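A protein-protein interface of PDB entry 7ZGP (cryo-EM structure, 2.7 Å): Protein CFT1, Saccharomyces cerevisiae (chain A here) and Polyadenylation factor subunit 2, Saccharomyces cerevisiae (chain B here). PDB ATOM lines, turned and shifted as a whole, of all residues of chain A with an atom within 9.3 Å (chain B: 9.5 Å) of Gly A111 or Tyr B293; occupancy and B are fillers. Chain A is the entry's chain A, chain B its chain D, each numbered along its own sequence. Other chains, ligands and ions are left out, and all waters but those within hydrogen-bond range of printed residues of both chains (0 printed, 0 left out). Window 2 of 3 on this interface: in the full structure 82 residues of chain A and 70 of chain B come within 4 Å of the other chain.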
ATOM      1  N   TYR A 105       4.291  20.708  -1.713  1.00  0.00           N
ATOM      2  CA  TYR A 105       5.686  20.396  -1.978  1.00  0.00           C
ATOM      3  C   TYR A 105       6.104  19.009  -1.522  1.00  0.00           C
ATOM      4  O   TYR A 105       7.231  18.604  -1.822  1.00  0.00           O
ATOM      5  CB  TYR A 105       6.608  21.425  -1.308  1.00  0.00           C
ATOM      6  CG  TYR A 105       6.427  22.827  -1.821  1.00  0.00           C
ATOM      7  CD1 TYR A 105       6.662  23.134  -3.150  1.00  0.00           C
ATOM      8  CD2 TYR A 105       6.020  23.845  -0.975  1.00  0.00           C
ATOM      9  CE1 TYR A 105       6.495  24.413  -3.622  1.00  0.00           C
ATOM     10  CE2 TYR A 105       5.853  25.127  -1.438  1.00  0.00           C
ATOM     11  CZ  TYR A 105       6.091  25.406  -2.762  1.00  0.00           C
ATOM     12  OH  TYR A 105       5.923  26.686  -3.223  1.00  0.00           O
ATOM     13  N   GLU A 106       5.249  18.276  -0.805  1.00  0.00           N
ATOM     14  CA  GLU A 106       5.641  16.959  -0.316  1.00  0.00           C
ATOM     15  C   GLU A 106       5.935  16.007  -1.468  1.00  0.00           C
ATOM     16  O   GLU A 106       6.889  15.227  -1.406  1.00  0.00           O
ATOM     17  CB  GLU A 106       4.558  16.384   0.594  1.00  0.00           C
ATOM     18  CG  GLU A 106       4.938  15.052   1.226  1.00  0.00           C
ATOM     19  CD  GLU A 106       3.959  14.604   2.291  1.00  0.00           C
ATOM     20  OE1 GLU A 106       3.080  15.405   2.670  1.00  0.00           O
ATOM     21  OE2 GLU A 106       4.070  13.449   2.753  1.00  0.00           O
ATOM     22  N   GLY A 107       5.132  16.062  -2.532  1.00  0.00           N
ATOM     23  CA  GLY A 107       5.370  15.180  -3.663  1.00  0.00           C
ATOM     24  C   GLY A 107       6.708  15.436  -4.328  1.00  0.00           C
ATOM     25  O   GLY A 107       7.473  14.507  -4.599  1.00  0.00           O
ATOM     26  N   LYS A 108       7.020  16.709  -4.580  1.00  0.00           N
ATOM     27  CA  LYS A 108       8.309  17.053  -5.171  1.00  0.00           C
ATOM     28  C   LYS A 108       9.455  16.715  -4.227  1.00  0.00           C
ATOM     29  O   LYS A 108      10.517  16.256  -4.666  1.00  0.00           O
ATOM     30  CB  LYS A 108       8.333  18.535  -5.543  1.00  0.00           C
ATOM     31  CG  LYS A 108       7.767  18.838  -6.918  1.00  0.00           C
ATOM     32  CD  LYS A 108       7.508  20.324  -7.092  1.00  0.00           C
ATOM     33  CE  LYS A 108       6.035  20.651  -6.911  1.00  0.00           C
ATOM     34  NZ  LYS A 108       5.723  22.053  -7.307  1.00  0.00           N
ATOM     35  N   PHE A 109       9.260  16.939  -2.925  1.00  0.00           N
ATOM     36  CA  PHE A 109      10.294  16.608  -1.951  1.00  0.00           C
ATOM     37  C   PHE A 109      10.598  15.114  -1.965  1.00  0.00           C
ATOM     38  O   PHE A 109      11.764  14.708  -1.973  1.00  0.00           O
ATOM     39  CB  PHE A 109       9.867  17.058  -0.553  1.00  0.00           C
ATOM     40  CG  PHE A 109      10.052  18.529  -0.297  1.00  0.00           C
ATOM     41  CD1 PHE A 109      10.316  19.405  -1.333  1.00  0.00           C
ATOM     42  CD2 PHE A 109       9.965  19.033   0.990  1.00  0.00           C
ATOM     43  CE1 PHE A 109      10.488  20.752  -1.092  1.00  0.00           C
ATOM     44  CE2 PHE A 109      10.134  20.380   1.235  1.00  0.00           C
ATOM     45  CZ  PHE A 109      10.395  21.239   0.193  1.00  0.00           C
ATOM     46  N   LYS A 110       9.556  14.277  -1.980  1.00  0.00           N
ATOM     47  CA  LYS A 110       9.769  12.835  -2.065  1.00  0.00           C
ATOM     48  C   LYS A 110      10.424  12.455  -3.384  1.00  0.00           C
ATOM     49  O   LYS A 110      11.279  11.563  -3.427  1.00  0.00           O
ATOM     50  CB  LYS A 110       8.446  12.089  -1.892  1.00  0.00           C
ATOM     51  CG  LYS A 110       7.723  12.378  -0.591  1.00  0.00           C
ATOM     52  CD  LYS A 110       7.494  11.115   0.217  1.00  0.00           C
ATOM     53  CE  LYS A 110       6.298  10.343  -0.311  1.00  0.00           C
ATOM     54  NZ  LYS A 110       5.017  10.965   0.120  1.00  0.00           N
ATOM     55  N   GLY A 111      10.030  13.115  -4.474  1.00  0.00           N
ATOM     56  CA  GLY A 111      10.644  12.832  -5.758  1.00  0.00           C
ATOM     57  C   GLY A 111      12.127  13.141  -5.794  1.00  0.00           C
ATOM     58  O   GLY A 111      12.894  12.437  -6.455  1.00  0.00           O
ATOM     59  N   LYS A 112      12.552  14.187  -5.090  1.00  0.00           N
ATOM     60  CA  LYS A 112      13.947  14.609  -5.102  1.00  0.00           C
ATOM     61  C   LYS A 112      14.727  14.159  -3.871  1.00  0.00           C
ATOM     62  O   LYS A 112      15.839  14.645  -3.650  1.00  0.00           O
ATOM     63  CB  LYS A 112      14.035  16.129  -5.245  1.00  0.00           C
ATOM     64  CG  LYS A 112      13.736  16.626  -6.645  1.00  0.00           C
ATOM     65  CD  LYS A 112      14.110  18.084  -6.812  1.00  0.00           C
ATOM     66  CE  LYS A 112      13.990  18.511  -8.263  1.00  0.00           C
ATOM     67  NZ  LYS A 112      14.420  19.918  -8.469  1.00  0.00           N
ATOM     68  N   SER A 113      14.182  13.247  -3.070  1.00  0.00           N
ATOM     69  CA  SER A 113      14.839  12.789  -1.853  1.00  0.00           C
ATOM     70  C   SER A 113      15.127  11.297  -1.943  1.00  0.00           C
ATOM     71  O   SER A 113      14.236  10.506  -2.267  1.00  0.00           O
ATOM     72  CB  SER A 113      13.984  13.078  -0.618  1.00  0.00           C
ATOM     73  OG  SER A 113      14.534  12.477   0.539  1.00  0.00           O
ATOM     74  N   LEU A 114      16.374  10.921  -1.655  1.00  0.00           N
ATOM     75  CA  LEU A 114      16.724   9.510  -1.540  1.00  0.00           C
ATOM     76  C   LEU A 114      16.260   8.919  -0.217  1.00  0.00           C
ATOM     77  O   LEU A 114      15.902   7.737  -0.160  1.00  0.00           O
ATOM     78  CB  LEU A 114      18.234   9.330  -1.691  1.00  0.00           C
ATOM     79  CG  LEU A 114      18.822   9.774  -3.029  1.00  0.00           C
ATOM     80  CD1 LEU A 114      20.327   9.578  -3.045  1.00  0.00           C
ATOM     81  CD2 LEU A 114      18.166   9.014  -4.166  1.00  0.00           C
ATOM     82  N   VAL A 115      16.261   9.717   0.845  1.00  0.00           N
ATOM     83  CA  VAL A 115      15.884   9.261   2.173  1.00  0.00           C
ATOM     84  C   VAL A 115      14.499   9.815   2.498  1.00  0.00           C
ATOM     85  O   VAL A 115      13.958  10.658   1.782  1.00  0.00           O
ATOM     86  CB  VAL A 115      16.926   9.675   3.236  1.00  0.00           C
ATOM     87  CG1 VAL A 115      16.753  11.139   3.614  1.00  0.00           C
ATOM     88  CG2 VAL A 115      16.861   8.771   4.460  1.00  0.00           C
ATOM     89  N   LEU A 117      11.637  12.014   4.151  1.00  0.00           N
ATOM     90  CA  LEU A 117      11.597  13.425   4.493  1.00  0.00           C
ATOM     91  C   LEU A 117      11.517  13.612   6.004  1.00  0.00           C
ATOM     92  O   LEU A 117      11.057  12.740   6.745  1.00  0.00           O
ATOM     93  CB  LEU A 117      10.399  14.106   3.835  1.00  0.00           C
ATOM     94  CG  LEU A 117      10.239  13.964   2.325  1.00  0.00           C
ATOM     95  CD1 LEU A 117       8.962  14.653   1.889  1.00  0.00           C
ATOM     96  CD2 LEU A 117      11.440  14.546   1.605  1.00  0.00           C
ATOM     97  N   ILE A 139      16.623  19.676   0.330  1.00  0.00           N
ATOM     98  CA  ILE A 139      15.750  20.015  -0.787  1.00  0.00           C
ATOM     99  C   ILE A 139      15.064  21.329  -0.457  1.00  0.00           C
ATOM    100  O   ILE A 139      14.386  21.444   0.570  1.00  0.00           O
ATOM    101  CB  ILE A 139      14.719  18.907  -1.066  1.00  0.00           C
ATOM    102  CG1 ILE A 139      15.401  17.648  -1.600  1.00  0.00           C
ATOM    103  CG2 ILE A 139      13.699  19.389  -2.069  1.00  0.00           C
ATOM    104  CD1 ILE A 139      15.462  16.517  -0.610  1.00  0.00           C
ATOM    105  N   VAL A 200      11.580  23.876  -7.005  1.00  0.00           N
ATOM    106  CA  VAL A 200      12.083  22.980  -5.971  1.00  0.00           C
ATOM    107  C   VAL A 200      13.379  22.361  -6.473  1.00  0.00           C
ATOM    108  O   VAL A 200      13.426  21.830  -7.587  1.00  0.00           O
ATOM    109  CB  VAL A 200      11.056  21.890  -5.618  1.00  0.00           C
ATOM    110  CG1 VAL A 200      11.663  20.876  -4.667  1.00  0.00           C
ATOM    111  CG2 VAL A 200       9.809  22.512  -5.016  1.00  0.00           C
ATOM    112  N   VAL A 202      17.478  20.590  -5.051  1.00  0.00           N
ATOM    113  CA  VAL A 202      18.361  20.114  -3.994  1.00  0.00           C
ATOM    114  C   VAL A 202      19.384  21.195  -3.673  1.00  0.00           C
ATOM    115  O   VAL A 202      19.734  22.021  -4.523  1.00  0.00           O
ATOM    116  CB  VAL A 202      19.041  18.795  -4.418  1.00  0.00           C
ATOM    117  CG1 VAL A 202      19.727  18.129  -3.233  1.00  0.00           C
ATOM    118  CG2 VAL A 202      18.027  17.858  -5.048  1.00  0.00           C
ATOM    119  N   MET B 231       6.435  -3.404  -3.193  1.00  0.00           N
ATOM    120  CA  MET B 231       5.686  -3.846  -4.356  1.00  0.00           C
ATOM    121  C   MET B 231       6.275  -5.142  -4.904  1.00  0.00           C
ATOM    122  O   MET B 231       7.240  -5.698  -4.372  1.00  0.00           O
ATOM    123  CB  MET B 231       5.665  -2.757  -5.429  1.00  0.00           C
ATOM    124  CG  MET B 231       6.991  -2.545  -6.132  1.00  0.00           C
ATOM    125  SD  MET B 231       7.364  -0.802  -6.387  1.00  0.00           S
ATOM    126  CE  MET B 231       8.882  -0.924  -7.324  1.00  0.00           C
ATOM    127  N   SER B 255      13.336  -5.166 -17.090  1.00  0.00           N
ATOM    128  CA  SER B 255      14.454  -4.286 -17.394  1.00  0.00           C
ATOM    129  C   SER B 255      15.745  -5.002 -17.033  1.00  0.00           C
ATOM    130  O   SER B 255      15.768  -5.883 -16.169  1.00  0.00           O
ATOM    131  CB  SER B 255      14.346  -2.951 -16.649  1.00  0.00           C
ATOM    132  OG  SER B 255      13.984  -3.148 -15.295  1.00  0.00           O
ATOM    133  N   GLY B 274      13.010   0.601  -0.353  1.00  0.00           N
ATOM    134  CA  GLY B 274      13.271  -0.059  -1.612  1.00  0.00           C
ATOM    135  C   GLY B 274      13.432   0.861  -2.799  1.00  0.00           C
ATOM    136  O   GLY B 274      13.533   0.371  -3.928  1.00  0.00           O
ATOM    137  N   ASN B 275      13.458   2.178  -2.584  1.00  0.00           N
ATOM    138  CA  ASN B 275      13.635   3.107  -3.696  1.00  0.00           C
ATOM    139  C   ASN B 275      14.990   2.927  -4.367  1.00  0.00           C
ATOM    140  O   ASN B 275      15.134   3.209  -5.562  1.00  0.00           O
ATOM    141  CB  ASN B 275      13.475   4.547  -3.211  1.00  0.00           C
ATOM    142  CG  ASN B 275      12.057   4.863  -2.779  1.00  0.00           C
ATOM    143  OD1 ASN B 275      11.094   4.366  -3.361  1.00  0.00           O
ATOM    144  ND2 ASN B 275      11.922   5.694  -1.753  1.00  0.00           N
ATOM    145  N   LEU B 276      15.988   2.470  -3.621  1.00  0.00           N
ATOM    146  CA  LEU B 276      17.316   2.215  -4.149  1.00  0.00           C
ATOM    147  C   LEU B 276      17.516   0.721  -4.372  1.00  0.00           C
ATOM    148  O   LEU B 276      16.752  -0.113  -3.885  1.00  0.00           O
ATOM    149  CB  LEU B 276      18.388   2.751  -3.196  1.00  0.00           C
ATOM    150  CG  LEU B 276      18.118   4.137  -2.610  1.00  0.00           C
ATOM    151  CD1 LEU B 276      19.124   4.469  -1.522  1.00  0.00           C
ATOM    152  CD2 LEU B 276      18.142   5.186  -3.703  1.00  0.00           C
ATOM    153  N   PHE B 289      21.401   1.976  -7.638  1.00  0.00           N
ATOM    154  CA  PHE B 289      20.493   2.407  -8.688  1.00  0.00           C
ATOM    155  C   PHE B 289      19.197   2.926  -8.083  1.00  0.00           C
ATOM    156  O   PHE B 289      18.684   2.363  -7.113  1.00  0.00           O
ATOM    157  CB  PHE B 289      20.186   1.264  -9.658  1.00  0.00           C
ATOM    158  CG  PHE B 289      21.408   0.634 -10.257  1.00  0.00           C
ATOM    159  CD1 PHE B 289      22.031   1.205 -11.352  1.00  0.00           C
ATOM    160  CD2 PHE B 289      21.931  -0.531  -9.725  1.00  0.00           C
ATOM    161  CE1 PHE B 289      23.153   0.627 -11.904  1.00  0.00           C
ATOM    162  CE2 PHE B 289      23.053  -1.112 -10.274  1.00  0.00           C
ATOM    163  CZ  PHE B 289      23.665  -0.534 -11.365  1.00  0.00           C
ATOM    164  N   ASP B 290      18.675   4.004  -8.663  1.00  0.00           N
ATOM    165  CA  ASP B 290      17.377   4.546  -8.280  1.00  0.00           C
ATOM    166  C   ASP B 290      16.315   3.882  -9.147  1.00  0.00           C
ATOM    167  O   ASP B 290      16.203   4.178 -10.340  1.00  0.00           O
ATOM    168  CB  ASP B 290      17.357   6.064  -8.442  1.00  0.00           C
ATOM    169  CG  ASP B 290      16.371   6.736  -7.507  1.00  0.00           C
ATOM    170  OD1 ASP B 290      15.214   6.273  -7.423  1.00  0.00           O
ATOM    171  OD2 ASP B 290      16.752   7.730  -6.857  1.00  0.00           O
ATOM    172  N   ILE B 291      15.537   2.976  -8.547  1.00  0.00           N
ATOM    173  CA  ILE B 291      14.540   2.236  -9.309  1.00  0.00           C
ATOM    174  C   ILE B 291      13.397   3.129  -9.769  1.00  0.00           C
ATOM    175  O   ILE B 291      12.666   2.764 -10.696  1.00  0.00           O
ATOM    176  CB  ILE B 291      13.997   1.056  -8.483  1.00  0.00           C
ATOM    177  CG1 ILE B 291      12.996   1.549  -7.442  1.00  0.00           C
ATOM    178  CG2 ILE B 291      15.135   0.315  -7.804  1.00  0.00           C
ATOM    179  CD1 ILE B 291      12.172   0.451  -6.839  1.00  0.00           C
ATOM    180  N   ARG B 292      13.224   4.297  -9.149  1.00  0.00           N
ATOM    181  CA  ARG B 292      12.140   5.200  -9.507  1.00  0.00           C
ATOM    182  C   ARG B 292      12.424   6.003 -10.768  1.00  0.00           C
ATOM    183  O   ARG B 292      11.510   6.659 -11.279  1.00  0.00           O
ATOM    184  CB  ARG B 292      11.855   6.163  -8.355  1.00  0.00           C
ATOM    185  CG  ARG B 292      11.402   5.494  -7.072  1.00  0.00           C
ATOM    186  CD  ARG B 292      11.401   6.485  -5.924  1.00  0.00           C
ATOM    187  NE  ARG B 292      12.615   7.291  -5.910  1.00  0.00           N
ATOM    188  CZ  ARG B 292      12.861   8.262  -5.041  1.00  0.00           C
ATOM    189  NH1 ARG B 292      11.996   8.575  -4.092  1.00  0.00           N
ATOM    190  NH2 ARG B 292      14.004   8.936  -5.129  1.00  0.00           N
ATOM    191  N   TYR B 293      13.651   5.971 -11.281  1.00  0.00           N
ATOM    192  CA  TYR B 293      14.062   6.812 -12.401  1.00  0.00           C
ATOM    193  C   TYR B 293      14.815   5.991 -13.438  1.00  0.00           C
ATOM    194  O   TYR B 293      15.893   6.367 -13.903  1.00  0.00           O
ATOM    195  CB  TYR B 293      14.897   7.984 -11.904  1.00  0.00           C
ATOM    196  CG  TYR B 293      14.150   8.851 -10.921  1.00  0.00           C
ATOM    197  CD1 TYR B 293      13.073   9.623 -11.331  1.00  0.00           C
ATOM    198  CD2 TYR B 293      14.507   8.883  -9.581  1.00  0.00           C
ATOM    199  CE1 TYR B 293      12.379  10.409 -10.439  1.00  0.00           C
ATOM    200  CE2 TYR B 293      13.818   9.668  -8.680  1.00  0.00           C
ATOM    201  CZ  TYR B 293      12.755  10.428  -9.115  1.00  0.00           C
ATOM    202  OH  TYR B 293      12.063  11.213  -8.222  1.00  0.00           O
ATOM    203  N   SER B 294      14.243   4.843 -13.804  1.00  0.00           N
ATOM    204  CA  SER B 294      14.784   3.976 -14.852  1.00  0.00           C
ATOM    205  C   SER B 294      16.198   3.507 -14.514  1.00  0.00           C
ATOM    206  O   SER B 294      17.127   3.631 -15.316  1.00  0.00           O
ATOM    207  CB  SER B 294      14.747   4.673 -16.215  1.00  0.00           C
ATOM    208  OG  SER B 294      15.831   5.573 -16.358  1.00  0.00           O
ATOM    209  N   MET B 295      16.351   2.956 -13.308  1.00  0.00           N
ATOM    210  CA  MET B 295      17.620   2.397 -12.840  1.00  0.00           C
ATOM    211  C   MET B 295      18.745   3.428 -12.931  1.00  0.00           C
ATOM    212  O   MET B 295      19.853   3.134 -13.382  1.00  0.00           O
ATOM    213  CB  MET B 295      17.982   1.131 -13.619  1.00  0.00           C
ATOM    214  CG  MET B 295      17.221  -0.110 -13.198  1.00  0.00           C
ATOM    215  SD  MET B 295      17.151  -0.337 -11.415  1.00  0.00           S
ATOM    216  CE  MET B 295      15.447  -0.846 -11.228  1.00  0.00           C
ATOM    217  N   LYS B 296      18.447   4.652 -12.504  1.00  0.00           N
ATOM    218  CA  LYS B 296      19.433   5.723 -12.571  1.00  0.00           C
ATOM    219  C   LYS B 296      20.609   5.417 -11.654  1.00  0.00           C
ATOM    220  O   LYS B 296      20.426   5.098 -10.477  1.00  0.00           O
ATOM    221  CB  LYS B 296      18.800   7.057 -12.186  1.00  0.00           C
ATOM    222  CG  LYS B 296      19.701   8.253 -12.441  1.00  0.00           C
ATOM    223  CD  LYS B 296      18.925   9.558 -12.388  1.00  0.00           C
ATOM    224  CE  LYS B 296      18.427   9.848 -10.984  1.00  0.00           C
ATOM    225  NZ  LYS B 296      17.478  10.995 -10.963  1.00  0.00           N
ATOM    226  N   GLU B 297      21.817   5.518 -12.198  1.00  0.00           N
ATOM    227  CA  GLU B 297      23.015   5.287 -11.403  1.00  0.00           C
ATOM    228  C   GLU B 297      23.227   6.437 -10.428  1.00  0.00           C
ATOM    229  O   GLU B 297      23.200   7.609 -10.816  1.00  0.00           O
ATOM    230  CB  GLU B 297      24.230   5.134 -12.313  1.00  0.00           C
ATOM    231  CG  GLU B 297      25.540   4.933 -11.573  1.00  0.00           C
ATOM    232  CD  GLU B 297      25.950   3.481 -11.504  1.00  0.00           C
ATOM    233  OE1 GLU B 297      25.528   2.701 -12.380  1.00  0.00           O
ATOM    234  OE2 GLU B 297      26.702   3.119 -10.577  1.00  0.00           O
ATOM    235  N   LEU B 298      23.441   6.098  -9.158  1.00  0.00           N
ATOM    236  CA  LEU B 298      23.700   7.084  -8.119  1.00  0.00           C
ATOM    237  C   LEU B 298      25.134   7.004  -7.614  1.00  0.00           C
ATOM    238  O   LEU B 298      25.846   8.011  -7.597  1.00  0.00           O
ATOM    239  CB  LEU B 298      22.717   6.894  -6.957  1.00  0.00           C
ATOM    240  CG  LEU B 298      21.230   7.008  -7.283  1.00  0.00           C
ATOM    241  CD1 LEU B 298      20.410   6.836  -6.023  1.00  0.00           C
ATOM    242  CD2 LEU B 298      20.926   8.341  -7.945  1.00  0.00           C
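The side-chain hydroxyl of Tyr B293 lies close to the backbone carbonyl oxygen of Gly A111, 2.3 Å away. The guanidinium group (NH2) of Arg B292 sits at hydrogen-bond distance from the backbone carbonyl oxygen (O) of Ser A113 (3.3 Å). O of Lys A110 lies within hydrogen-bond range of NH1 of Arg B292 (3.1 Å).
OE2 of Glu A106 lies within salt-bridge range of NZ of Lys A110, at 3.7 Å. The guanidinium group of Arg B292 is in salt-bridge range of the side-chain carboxylate of Asp B290, 3.2 Å away. OG of Ser A113 lies within hydrogen-bond range of N of Val A115, 3.3 Å away. O of Asp B290 sits at hydrogen-bond distance from N of Met B295 (3.2 Å). O of Lys B296 is in hydrogen-bond range of N of Asp B290.
Of the 15 printed residues of chain A, 4 touch a printed residue of chain B. Along chain B the printed residues that touch a printed residue of chain A span positions 276 to 298. Among the printed residues, 7 pairs touch across the chains.
Glu A106 touches none of the printed residues of chain B. Gly A111 touches two residues of chain B. Of the printed residues of chain B, Ser A113 touches Arg B292. Of the printed residues of chain B, Leu A114 touches Leu B276, Asp B290 and Leu B298. Met B231 touches none of the printed residues of chain A. Of chain A, only Lys A110, Gly A111 and Ser A113 come within 4 Å of Arg B292. No residue of chain A comes within 4 Å of Ser B294. Of the printed residues of chain A, Leu B298 touches Leu A114 (3.6 Å). The nearest residue of chain A that does not touch Tyr B293 is Lys A112 (4.3 Å).
Arg B292 touches Gly A111. Leu B276 touches Leu A114 (CD2 to CD2, 3.9 Å). Leu A114 touches Asp B290 (CD2 to OD2, 3.3 Å). Leu A114 touches Leu B298.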
